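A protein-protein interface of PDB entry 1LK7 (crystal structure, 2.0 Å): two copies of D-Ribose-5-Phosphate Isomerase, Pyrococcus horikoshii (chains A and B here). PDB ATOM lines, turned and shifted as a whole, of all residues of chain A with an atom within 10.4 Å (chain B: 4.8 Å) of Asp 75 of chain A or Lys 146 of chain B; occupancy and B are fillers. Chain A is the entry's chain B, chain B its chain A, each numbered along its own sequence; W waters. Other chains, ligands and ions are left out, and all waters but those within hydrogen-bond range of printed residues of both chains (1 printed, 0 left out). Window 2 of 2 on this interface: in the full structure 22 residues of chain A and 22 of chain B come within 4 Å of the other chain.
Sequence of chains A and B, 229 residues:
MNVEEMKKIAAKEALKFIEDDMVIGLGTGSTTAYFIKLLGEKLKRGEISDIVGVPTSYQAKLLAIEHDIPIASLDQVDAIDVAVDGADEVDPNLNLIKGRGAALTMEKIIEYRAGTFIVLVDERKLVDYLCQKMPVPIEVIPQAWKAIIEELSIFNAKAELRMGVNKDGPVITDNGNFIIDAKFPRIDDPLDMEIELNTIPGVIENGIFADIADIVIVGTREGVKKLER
The backbone carbonyl oxygen (O) of Gln 143 of chain B sits at hydrogen-bond distance from the backbone NH (N) of Asp 75 of chain A, at 3.4 Å. The side-chain amide oxygen of Gln 143 of chain B lies close to the side-chain sulfur of Met 106 of chain A (3.6 Å). OD2 of Asp 75 of chain A lies within hydrogen-bond range of NE1 of Trp 145 of chain B, 3.0 Å away. The side-chain amide oxygen (OE1) of Gln 143 of chain B sits at hydrogen-bond distance from the backbone NH (N) of Leu 74 of chain A (3.0 Å).
The side-chain hydroxyl (OG) of Ser 73 of chain A sits at hydrogen-bond distance from the side-chain carboxylate (OD1) of Asp 75 of chain A (2.9 Å). OE2 of Glu 150 of chain B is in salt-bridge range of NZ of Lys 146 of chain B (3.8 Å). The backbone carbonyl oxygen (O) of Ile 109 of chain A sits at hydrogen-bond distance from the guanidinium group (NH1) of Arg 113 of chain A. The backbone NH (N) of Ser 73 of chain A sits close to the side-chain amide nitrogen (NE2) of Gln 76 of chain A, at 3.0 Å.
Among the printed residues, pairs that only touch across the chains: Ser 73 of chain A with Gln 143 of chain B (3.5 Å), Asp 75 of chain A with Lys 146 of chain B (3.7 Å), Arg 113 of chain A with Ala 147 of chain B (3.7 Å) and Arg 113 of chain A with Ile 148 of chain B (3.8 Å).
Of chain B, only Gln 143 (3.4 Å), Trp 145 (3.0 Å) and Lys 146 (3.7 Å) come within 4 Å of Asp 75 of chain A. Printed residues of chain A within 4 Å of Lys 146 of chain B: Asp 75 (3.7 Å). Ala 144 of chain B touches none of the printed residues of chain A. Of chain A, only Asp 75 comes within 4 Å of Trp 145 of chain B. No residue of chain A comes within 4 Å of Ile 149 of chain B. Of the printed residues of chain B, Arg 113 of chain A touches Ala 147 (3.7 Å) and Ile 148 (3.8 Å). Printed residues of chain B within 4 Å of Ser 73 of chain A: Gln 143 (3.5 Å). Of the printed residues of chain B, Leu 74 of chain A touches Gln 143. Of the printed residues of chain B, Met 106 of chain A touches Gln 143. Gln 76 of chain A touches none of the printed residues of chain B. Ile 80 of chain A touches none of the printed residues of chain B. The nearest residue of chain A that does not touch Lys 146 of chain B is Val 77 of chain A (4.9 Å).
Of the 8 printed residues of chain B, 5 touch a printed residue of chain A. Hydrophobic or aromatic side chains of chain B within 4 Å of the printed part of chain A: Trp 145, Ala 147 and Ile 148. Among the printed residues, 8 pairs touch across the chains. Among the printed residues, no Asp or Glu carboxylate lies within 4 Å of a Lys or Arg side-chain nitrogen of the other chain.
No position is printed for both chains. Of the 8 pairs that touch across the chains among the printed residues, none has its exchanged pair printed and touching as well.
Water W1 bridges the side-chain amide oxygen of Gln 143 of chain B (2.7 Å) and the backbone carbonyl oxygen of Pro 55 of chain A (2.8 Å).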
ATOM      1  N   VAL A  23      13.814  27.923 -17.341  1.00  0.00           N
ATOM      2  CA  VAL A  23      12.748  28.217 -16.402  1.00  0.00           C
ATOM      3  C   VAL A  23      12.897  27.159 -15.294  1.00  0.00           C
ATOM      4  O   VAL A  23      12.883  25.961 -15.575  1.00  0.00           O
ATOM      5  CB  VAL A  23      11.366  28.115 -17.056  1.00  0.00           C
ATOM      6  CG1 VAL A  23      10.254  28.342 -16.022  1.00  0.00           C
ATOM      7  CG2 VAL A  23      11.229  29.086 -18.165  1.00  0.00           C
ATOM      8  N   VAL A  52      14.381  32.295 -15.216  1.00  0.00           N
ATOM      9  CA  VAL A  52      13.104  32.693 -14.630  1.00  0.00           C
ATOM     10  C   VAL A  52      12.714  31.629 -13.607  1.00  0.00           C
ATOM     11  O   VAL A  52      12.758  30.460 -13.924  1.00  0.00           O
ATOM     12  CB  VAL A  52      11.991  32.823 -15.699  1.00  0.00           C
ATOM     13  CG1 VAL A  52      10.699  33.215 -15.037  1.00  0.00           C
ATOM     14  CG2 VAL A  52      12.351  33.898 -16.739  1.00  0.00           C
ATOM     15  N   GLY A  53      12.393  32.026 -12.378  1.00  0.00           N
ATOM     16  CA  GLY A  53      11.999  31.083 -11.356  1.00  0.00           C
ATOM     17  C   GLY A  53      10.488  30.977 -11.270  1.00  0.00           C
ATOM     18  O   GLY A  53       9.777  31.972 -11.474  1.00  0.00           O
ATOM     19  N   VAL A  54       9.981  29.789 -10.935  1.00  0.00           N
ATOM     20  CA  VAL A  54       8.545  29.612 -10.738  1.00  0.00           C
ATOM     21  C   VAL A  54       8.418  29.066  -9.344  1.00  0.00           C
ATOM     22  O   VAL A  54       8.692  27.903  -9.092  1.00  0.00           O
ATOM     23  CB  VAL A  54       7.926  28.678 -11.769  1.00  0.00           C
ATOM     24  CG1 VAL A  54       6.444  28.472 -11.523  1.00  0.00           C
ATOM     25  CG2 VAL A  54       8.135  29.219 -13.159  1.00  0.00           C
ATOM     26  N   PRO A  55       8.015  29.915  -8.421  1.00  0.00           N
ATOM     27  CA  PRO A  55       8.016  29.526  -7.021  1.00  0.00           C
ATOM     28  C   PRO A  55       6.878  28.586  -6.627  1.00  0.00           C
ATOM     29  O   PRO A  55       5.774  28.649  -7.153  1.00  0.00           O
ATOM     30  CB  PRO A  55       7.930  30.867  -6.295  1.00  0.00           C
ATOM     31  CG  PRO A  55       7.208  31.742  -7.248  1.00  0.00           C
ATOM     32  CD  PRO A  55       7.549  31.287  -8.626  1.00  0.00           C
ATOM     33  N   ILE A  71      10.766  36.121 -11.442  1.00  0.00           N
ATOM     34  CA  ILE A  71       9.869  34.996 -11.249  1.00  0.00           C
ATOM     35  C   ILE A  71       8.587  35.130 -12.055  1.00  0.00           C
ATOM     36  O   ILE A  71       8.264  36.200 -12.557  1.00  0.00           O
ATOM     37  CB  ILE A  71       9.500  34.856  -9.780  1.00  0.00           C
ATOM     38  CG1 ILE A  71       8.941  36.164  -9.260  1.00  0.00           C
ATOM     39  CG2 ILE A  71      10.691  34.402  -8.930  1.00  0.00           C
ATOM     40  CD1 ILE A  71       8.275  36.004  -7.938  1.00  0.00           C
ATOM     41  N   ALA A  72       7.849  34.027 -12.122  1.00  0.00           N
ATOM     42  CA  ALA A  72       6.597  33.950 -12.852  1.00  0.00           C
ATOM     43  C   ALA A  72       5.799  32.795 -12.264  1.00  0.00           C
ATOM     44  O   ALA A  72       6.378  31.868 -11.682  1.00  0.00           O
ATOM     45  CB  ALA A  72       6.854  33.680 -14.296  1.00  0.00           C
ATOM     46  N   SER A  73       4.481  32.874 -12.420  1.00  0.00           N
ATOM     47  CA  SER A  73       3.598  31.785 -12.071  1.00  0.00           C
ATOM     48  C   SER A  73       3.571  30.780 -13.259  1.00  0.00           C
ATOM     49  O   SER A  73       3.976  31.092 -14.392  1.00  0.00           O
ATOM     50  CB  SER A  73       2.220  32.332 -11.648  1.00  0.00           C
ATOM     51  OG  SER A  73       1.588  33.010 -12.722  1.00  0.00           O
ATOM     52  N   LEU A  74       3.113  29.563 -13.004  1.00  0.00           N
ATOM     53  CA  LEU A  74       3.181  28.521 -14.019  1.00  0.00           C
ATOM     54  C   LEU A  74       2.533  28.910 -15.333  1.00  0.00           C
ATOM     55  O   LEU A  74       3.049  28.553 -16.402  1.00  0.00           O
ATOM     56  CB  LEU A  74       2.543  27.232 -13.511  1.00  0.00           C
ATOM     57  CG  LEU A  74       2.552  26.074 -14.501  1.00  0.00           C
ATOM     58  CD1 LEU A  74       3.955  25.616 -14.782  1.00  0.00           C
ATOM     59  CD2 LEU A  74       1.690  24.927 -13.980  1.00  0.00           C
ATOM     60  N   ASP A  75       1.428  29.648 -15.275  1.00  0.00           N
ATOM     61  CA  ASP A  75       0.698  29.956 -16.501  1.00  0.00           C
ATOM     62  C   ASP A  75       1.344  31.072 -17.316  1.00  0.00           C
ATOM     63  O   ASP A  75       0.875  31.413 -18.399  1.00  0.00           O
ATOM     64  CB  ASP A  75      -0.789  30.259 -16.241  1.00  0.00           C
ATOM     65  CG  ASP A  75      -1.002  31.441 -15.357  1.00  0.00           C
ATOM     66  OD1 ASP A  75      -0.325  31.566 -14.306  1.00  0.00           O
ATOM     67  OD2 ASP A  75      -1.853  32.307 -15.621  1.00  0.00           O
ATOM     68  N   GLN A  76       2.411  31.641 -16.782  1.00  0.00           N
ATOM     69  CA  GLN A  76       3.163  32.679 -17.476  1.00  0.00           C
ATOM     70  C   GLN A  76       4.253  32.106 -18.348  1.00  0.00           C
ATOM     71  O   GLN A  76       4.778  32.794 -19.226  1.00  0.00           O
ATOM     72  CB  GLN A  76       3.861  33.591 -16.463  1.00  0.00           C
ATOM     73  CG  GLN A  76       3.119  34.811 -16.047  1.00  0.00           C
ATOM     74  CD  GLN A  76       3.886  35.557 -14.998  1.00  0.00           C
ATOM     75  OE1 GLN A  76       4.816  36.302 -15.305  1.00  0.00           O
ATOM     76  NE2 GLN A  76       3.512  35.358 -13.753  1.00  0.00           N
ATOM     77  N   VAL A  77       4.616  30.852 -18.101  1.00  0.00           N
ATOM     78  CA  VAL A  77       5.725  30.240 -18.830  1.00  0.00           C
ATOM     79  C   VAL A  77       5.332  29.061 -19.720  1.00  0.00           C
ATOM     80  O   VAL A  77       4.322  28.403 -19.484  1.00  0.00           O
ATOM     81  CB  VAL A  77       6.821  29.792 -17.859  1.00  0.00           C
ATOM     82  CG1 VAL A  77       7.217  30.941 -16.961  1.00  0.00           C
ATOM     83  CG2 VAL A  77       6.365  28.593 -17.036  1.00  0.00           C
ATOM     84  N   ASP A  78       6.153  28.792 -20.735  1.00  0.00           N
ATOM     85  CA  ASP A  78       5.877  27.725 -21.688  1.00  0.00           C
ATOM     86  C   ASP A  78       6.251  26.348 -21.147  1.00  0.00           C
ATOM     87  O   ASP A  78       5.633  25.344 -21.504  1.00  0.00           O
ATOM     88  CB  ASP A  78       6.648  27.964 -22.982  1.00  0.00           C
ATOM     89  CG  ASP A  78       6.314  29.287 -23.631  1.00  0.00           C
ATOM     90  OD1 ASP A  78       5.127  29.697 -23.614  1.00  0.00           O
ATOM     91  OD2 ASP A  78       7.195  29.980 -24.198  1.00  0.00           O
ATOM     92  N   ALA A  79       7.239  26.311 -20.259  1.00  0.00           N
ATOM     93  CA  ALA A  79       7.710  25.062 -19.723  1.00  0.00           C
ATOM     94  C   ALA A  79       8.576  25.280 -18.489  1.00  0.00           C
ATOM     95  O   ALA A  79       9.078  26.373 -18.270  1.00  0.00           O
ATOM     96  CB  ALA A  79       8.512  24.334 -20.798  1.00  0.00           C
ATOM     97  N   ILE A  80       8.663  24.237 -17.665  1.00  0.00           N
ATOM     98  CA  ILE A  80       9.588  24.148 -16.563  1.00  0.00           C
ATOM     99  C   ILE A  80      10.737  23.211 -16.972  1.00  0.00           C
ATOM    100  O   ILE A  80      10.545  22.005 -17.105  1.00  0.00           O
ATOM    101  CB  ILE A  80       8.895  23.579 -15.327  1.00  0.00           C
ATOM    102  CG1 ILE A  80       7.670  24.431 -14.956  1.00  0.00           C
ATOM    103  CG2 ILE A  80       9.870  23.524 -14.148  1.00  0.00           C
ATOM    104  CD1 ILE A  80       8.019  25.709 -14.270  1.00  0.00           C
ATOM    105  N   MET A 106       1.282  23.341  -4.739  1.00  0.00           N
ATOM    106  CA  MET A 106       1.962  24.030  -5.835  1.00  0.00           C
ATOM    107  C   MET A 106       3.270  23.297  -6.221  1.00  0.00           C
ATOM    108  O   MET A 106       3.689  23.335  -7.366  1.00  0.00           O
ATOM    109  CB  MET A 106       2.232  25.488  -5.499  1.00  0.00           C
ATOM    110  CG  MET A 106       2.543  26.333  -6.760  1.00  0.00           C
ATOM    111  SD  MET A 106       1.157  26.515  -7.942  1.00  0.00           S
ATOM    112  CE  MET A 106      -0.159  26.456  -6.860  1.00  0.00           C
ATOM    113  N   ILE A 109       2.327  20.714  -8.559  1.00  0.00           N
ATOM    114  CA  ILE A 109       1.873  21.288  -9.806  1.00  0.00           C
ATOM    115  C   ILE A 109       3.052  21.654 -10.719  1.00  0.00           C
ATOM    116  O   ILE A 109       3.012  21.428 -11.924  1.00  0.00           O
ATOM    117  CB  ILE A 109       0.981  22.538  -9.544  1.00  0.00           C
ATOM    118  CG1 ILE A 109      -0.439  22.094  -9.162  1.00  0.00           C
ATOM    119  CG2 ILE A 109       0.951  23.421 -10.756  1.00  0.00           C
ATOM    120  CD1 ILE A 109      -1.250  23.228  -8.484  1.00  0.00           C
ATOM    121  N   ILE A 110       4.064  22.244 -10.142  1.00  0.00           N
ATOM    122  CA  ILE A 110       5.260  22.649 -10.858  1.00  0.00           C
ATOM    123  C   ILE A 110       6.213  21.508 -11.179  1.00  0.00           C
ATOM    124  O   ILE A 110       6.631  21.351 -12.313  1.00  0.00           O
ATOM    125  CB  ILE A 110       5.944  23.706 -10.019  1.00  0.00           C
ATOM    126  CG1 ILE A 110       5.067  24.964 -10.044  1.00  0.00           C
ATOM    127  CG2 ILE A 110       7.325  24.050 -10.560  1.00  0.00           C
ATOM    128  CD1 ILE A 110       5.332  25.876  -8.913  1.00  0.00           C
ATOM    129  N   ARG A 113       5.487  19.051 -14.018  1.00  0.00           N
ATOM    130  CA  ARG A 113       5.738  19.577 -15.342  1.00  0.00           C
ATOM    131  C   ARG A 113       7.203  19.824 -15.675  1.00  0.00           C
ATOM    132  O   ARG A 113       7.496  20.294 -16.772  1.00  0.00           O
ATOM    133  CB  ARG A 113       4.960  20.883 -15.532  1.00  0.00           C
ATOM    134  CG  ARG A 113       3.542  20.605 -16.000  1.00  0.00           C
ATOM    135  CD  ARG A 113       2.480  21.282 -15.190  1.00  0.00           C
ATOM    136  NE  ARG A 113       1.166  20.712 -15.440  1.00  0.00           N
ATOM    137  CZ  ARG A 113       0.255  20.521 -14.503  1.00  0.00           C
ATOM    138  NH1 ARG A 113       0.517  20.856 -13.251  1.00  0.00           N
ATOM    139  NH2 ARG A 113      -0.923  19.989 -14.816  1.00  0.00           N
ATOM    140  N   GLN B 143      -3.233  28.834 -11.112  1.00  0.00           N
ATOM    141  CA  GLN B 143      -2.049  28.929 -11.962  1.00  0.00           C
ATOM    142  C   GLN B 143      -1.814  27.724 -12.887  1.00  0.00           C
ATOM    143  O   GLN B 143      -0.976  27.801 -13.787  1.00  0.00           O
ATOM    144  CB  GLN B 143      -0.802  29.302 -11.143  1.00  0.00           C
ATOM    145  CG  GLN B 143      -0.139  28.232 -10.329  1.00  0.00           C
ATOM    146  CD  GLN B 143       1.133  28.751  -9.608  1.00  0.00           C
ATOM    147  OE1 GLN B 143       2.153  29.114 -10.248  1.00  0.00           O
ATOM    148  NE2 GLN B 143       1.077  28.755  -8.268  1.00  0.00           N
ATOM    149  N   ALA B 144      -2.571  26.649 -12.692  1.00  0.00           N
ATOM    150  CA  ALA B 144      -2.401  25.429 -13.492  1.00  0.00           C
ATOM    151  C   ALA B 144      -3.371  25.385 -14.639  1.00  0.00           C
ATOM    152  O   ALA B 144      -3.383  24.437 -15.423  1.00  0.00           O
ATOM    153  CB  ALA B 144      -2.611  24.168 -12.592  1.00  0.00           C
ATOM    154  N   TRP B 145      -4.180  26.426 -14.774  1.00  0.00           N
ATOM    155  CA  TRP B 145      -5.218  26.403 -15.772  1.00  0.00           C
ATOM    156  C   TRP B 145      -4.737  26.124 -17.205  1.00  0.00           C
ATOM    157  O   TRP B 145      -5.259  25.237 -17.866  1.00  0.00           O
ATOM    158  CB  TRP B 145      -6.075  27.657 -15.686  1.00  0.00           C
ATOM    159  CG  TRP B 145      -5.449  28.828 -16.303  1.00  0.00           C
ATOM    160  CD1 TRP B 145      -4.522  29.650 -15.758  1.00  0.00           C
ATOM    161  CD2 TRP B 145      -5.643  29.261 -17.637  1.00  0.00           C
ATOM    162  NE1 TRP B 145      -4.170  30.627 -16.659  1.00  0.00           N
ATOM    163  CE2 TRP B 145      -4.861  30.415 -17.822  1.00  0.00           C
ATOM    164  CE3 TRP B 145      -6.444  28.815 -18.691  1.00  0.00           C
ATOM    165  CZ2 TRP B 145      -4.816  31.093 -19.032  1.00  0.00           C
ATOM    166  CZ3 TRP B 145      -6.407  29.507 -19.906  1.00  0.00           C
ATOM    167  CH2 TRP B 145      -5.591  30.620 -20.063  1.00  0.00           C
ATOM    168  N   LYS B 146      -3.704  26.818 -17.653  1.00  0.00           N
ATOM    169  CA  LYS B 146      -3.315  26.732 -19.049  1.00  0.00           C
ATOM    170  C   LYS B 146      -2.693  25.373 -19.359  1.00  0.00           C
ATOM    171  O   LYS B 146      -2.917  24.750 -20.418  1.00  0.00           O
ATOM    172  CB  LYS B 146      -2.354  27.877 -19.367  1.00  0.00           C
ATOM    173  CG  LYS B 146      -1.309  27.537 -20.439  1.00  0.00           C
ATOM    174  CD  LYS B 146      -0.411  28.736 -20.648  1.00  0.00           C
ATOM    175  CE  LYS B 146      -1.150  29.837 -21.363  1.00  0.00           C
ATOM    176  NZ  LYS B 146      -1.133  29.685 -22.844  1.00  0.00           N
ATOM    177  N   ALA B 147      -1.903  24.889 -18.430  1.00  0.00           N
ATOM    178  CA  ALA B 147      -1.205  23.631 -18.634  1.00  0.00           C
ATOM    179  C   ALA B 147      -2.207  22.491 -18.680  1.00  0.00           C
ATOM    180  O   ALA B 147      -2.064  21.530 -19.433  1.00  0.00           O
ATOM    181  CB  ALA B 147      -0.237  23.410 -17.523  1.00  0.00           C
ATOM    182  N   ILE B 148      -3.226  22.594 -17.836  1.00  0.00           N
ATOM    183  CA  ILE B 148      -4.208  21.554 -17.772  1.00  0.00           C
ATOM    184  C   ILE B 148      -4.951  21.528 -19.068  1.00  0.00           C
ATOM    185  O   ILE B 148      -5.199  20.453 -19.616  1.00  0.00           O
ATOM    186  CB  ILE B 148      -5.157  21.768 -16.605  1.00  0.00           C
ATOM    187  CG1 ILE B 148      -4.452  21.362 -15.322  1.00  0.00           C
ATOM    188  CG2 ILE B 148      -6.399  20.922 -16.800  1.00  0.00           C
ATOM    189  CD1 ILE B 148      -5.109  21.865 -14.052  1.00  0.00           C
ATOM    190  N   ILE B 149      -5.305  22.705 -19.575  1.00  0.00           N
ATOM    191  CA  ILE B 149      -6.048  22.738 -20.820  1.00  0.00           C
ATOM    192  C   ILE B 149      -5.219  22.020 -21.912  1.00  0.00           C
ATOM    193  O   ILE B 149      -5.713  21.131 -22.604  1.00  0.00           O
ATOM    194  CB  ILE B 149      -6.350  24.141 -21.252  1.00  0.00           C
ATOM    195  CG1 ILE B 149      -7.531  24.655 -20.450  1.00  0.00           C
ATOM    196  CG2 ILE B 149      -6.683  24.191 -22.729  1.00  0.00           C
ATOM    197  CD1 ILE B 149      -7.866  26.069 -20.734  1.00  0.00           C
ATOM    198  N   GLU B 150      -3.965  22.448 -22.041  1.00  0.00           N
ATOM    199  CA  GLU B 150      -3.042  21.909 -23.029  1.00  0.00           C
ATOM    200  C   GLU B 150      -2.822  20.423 -22.804  1.00  0.00           C
ATOM    201  O   GLU B 150      -2.694  19.665 -23.773  1.00  0.00           O
ATOM    202  CB  GLU B 150      -1.718  22.686 -22.994  1.00  0.00           C
ATOM    203  CG  GLU B 150      -1.890  24.186 -23.252  1.00  0.00           C
ATOM    204  CD  GLU B 150      -0.633  25.006 -22.981  1.00  0.00           C
ATOM    205  OE1 GLU B 150       0.159  24.616 -22.095  1.00  0.00           O
ATOM    206  OE2 GLU B 150      -0.436  26.035 -23.671  1.00  0.00           O
HETATM  207  O   HOH W   1       4.244  30.108  -8.934  1.00  0.00           O
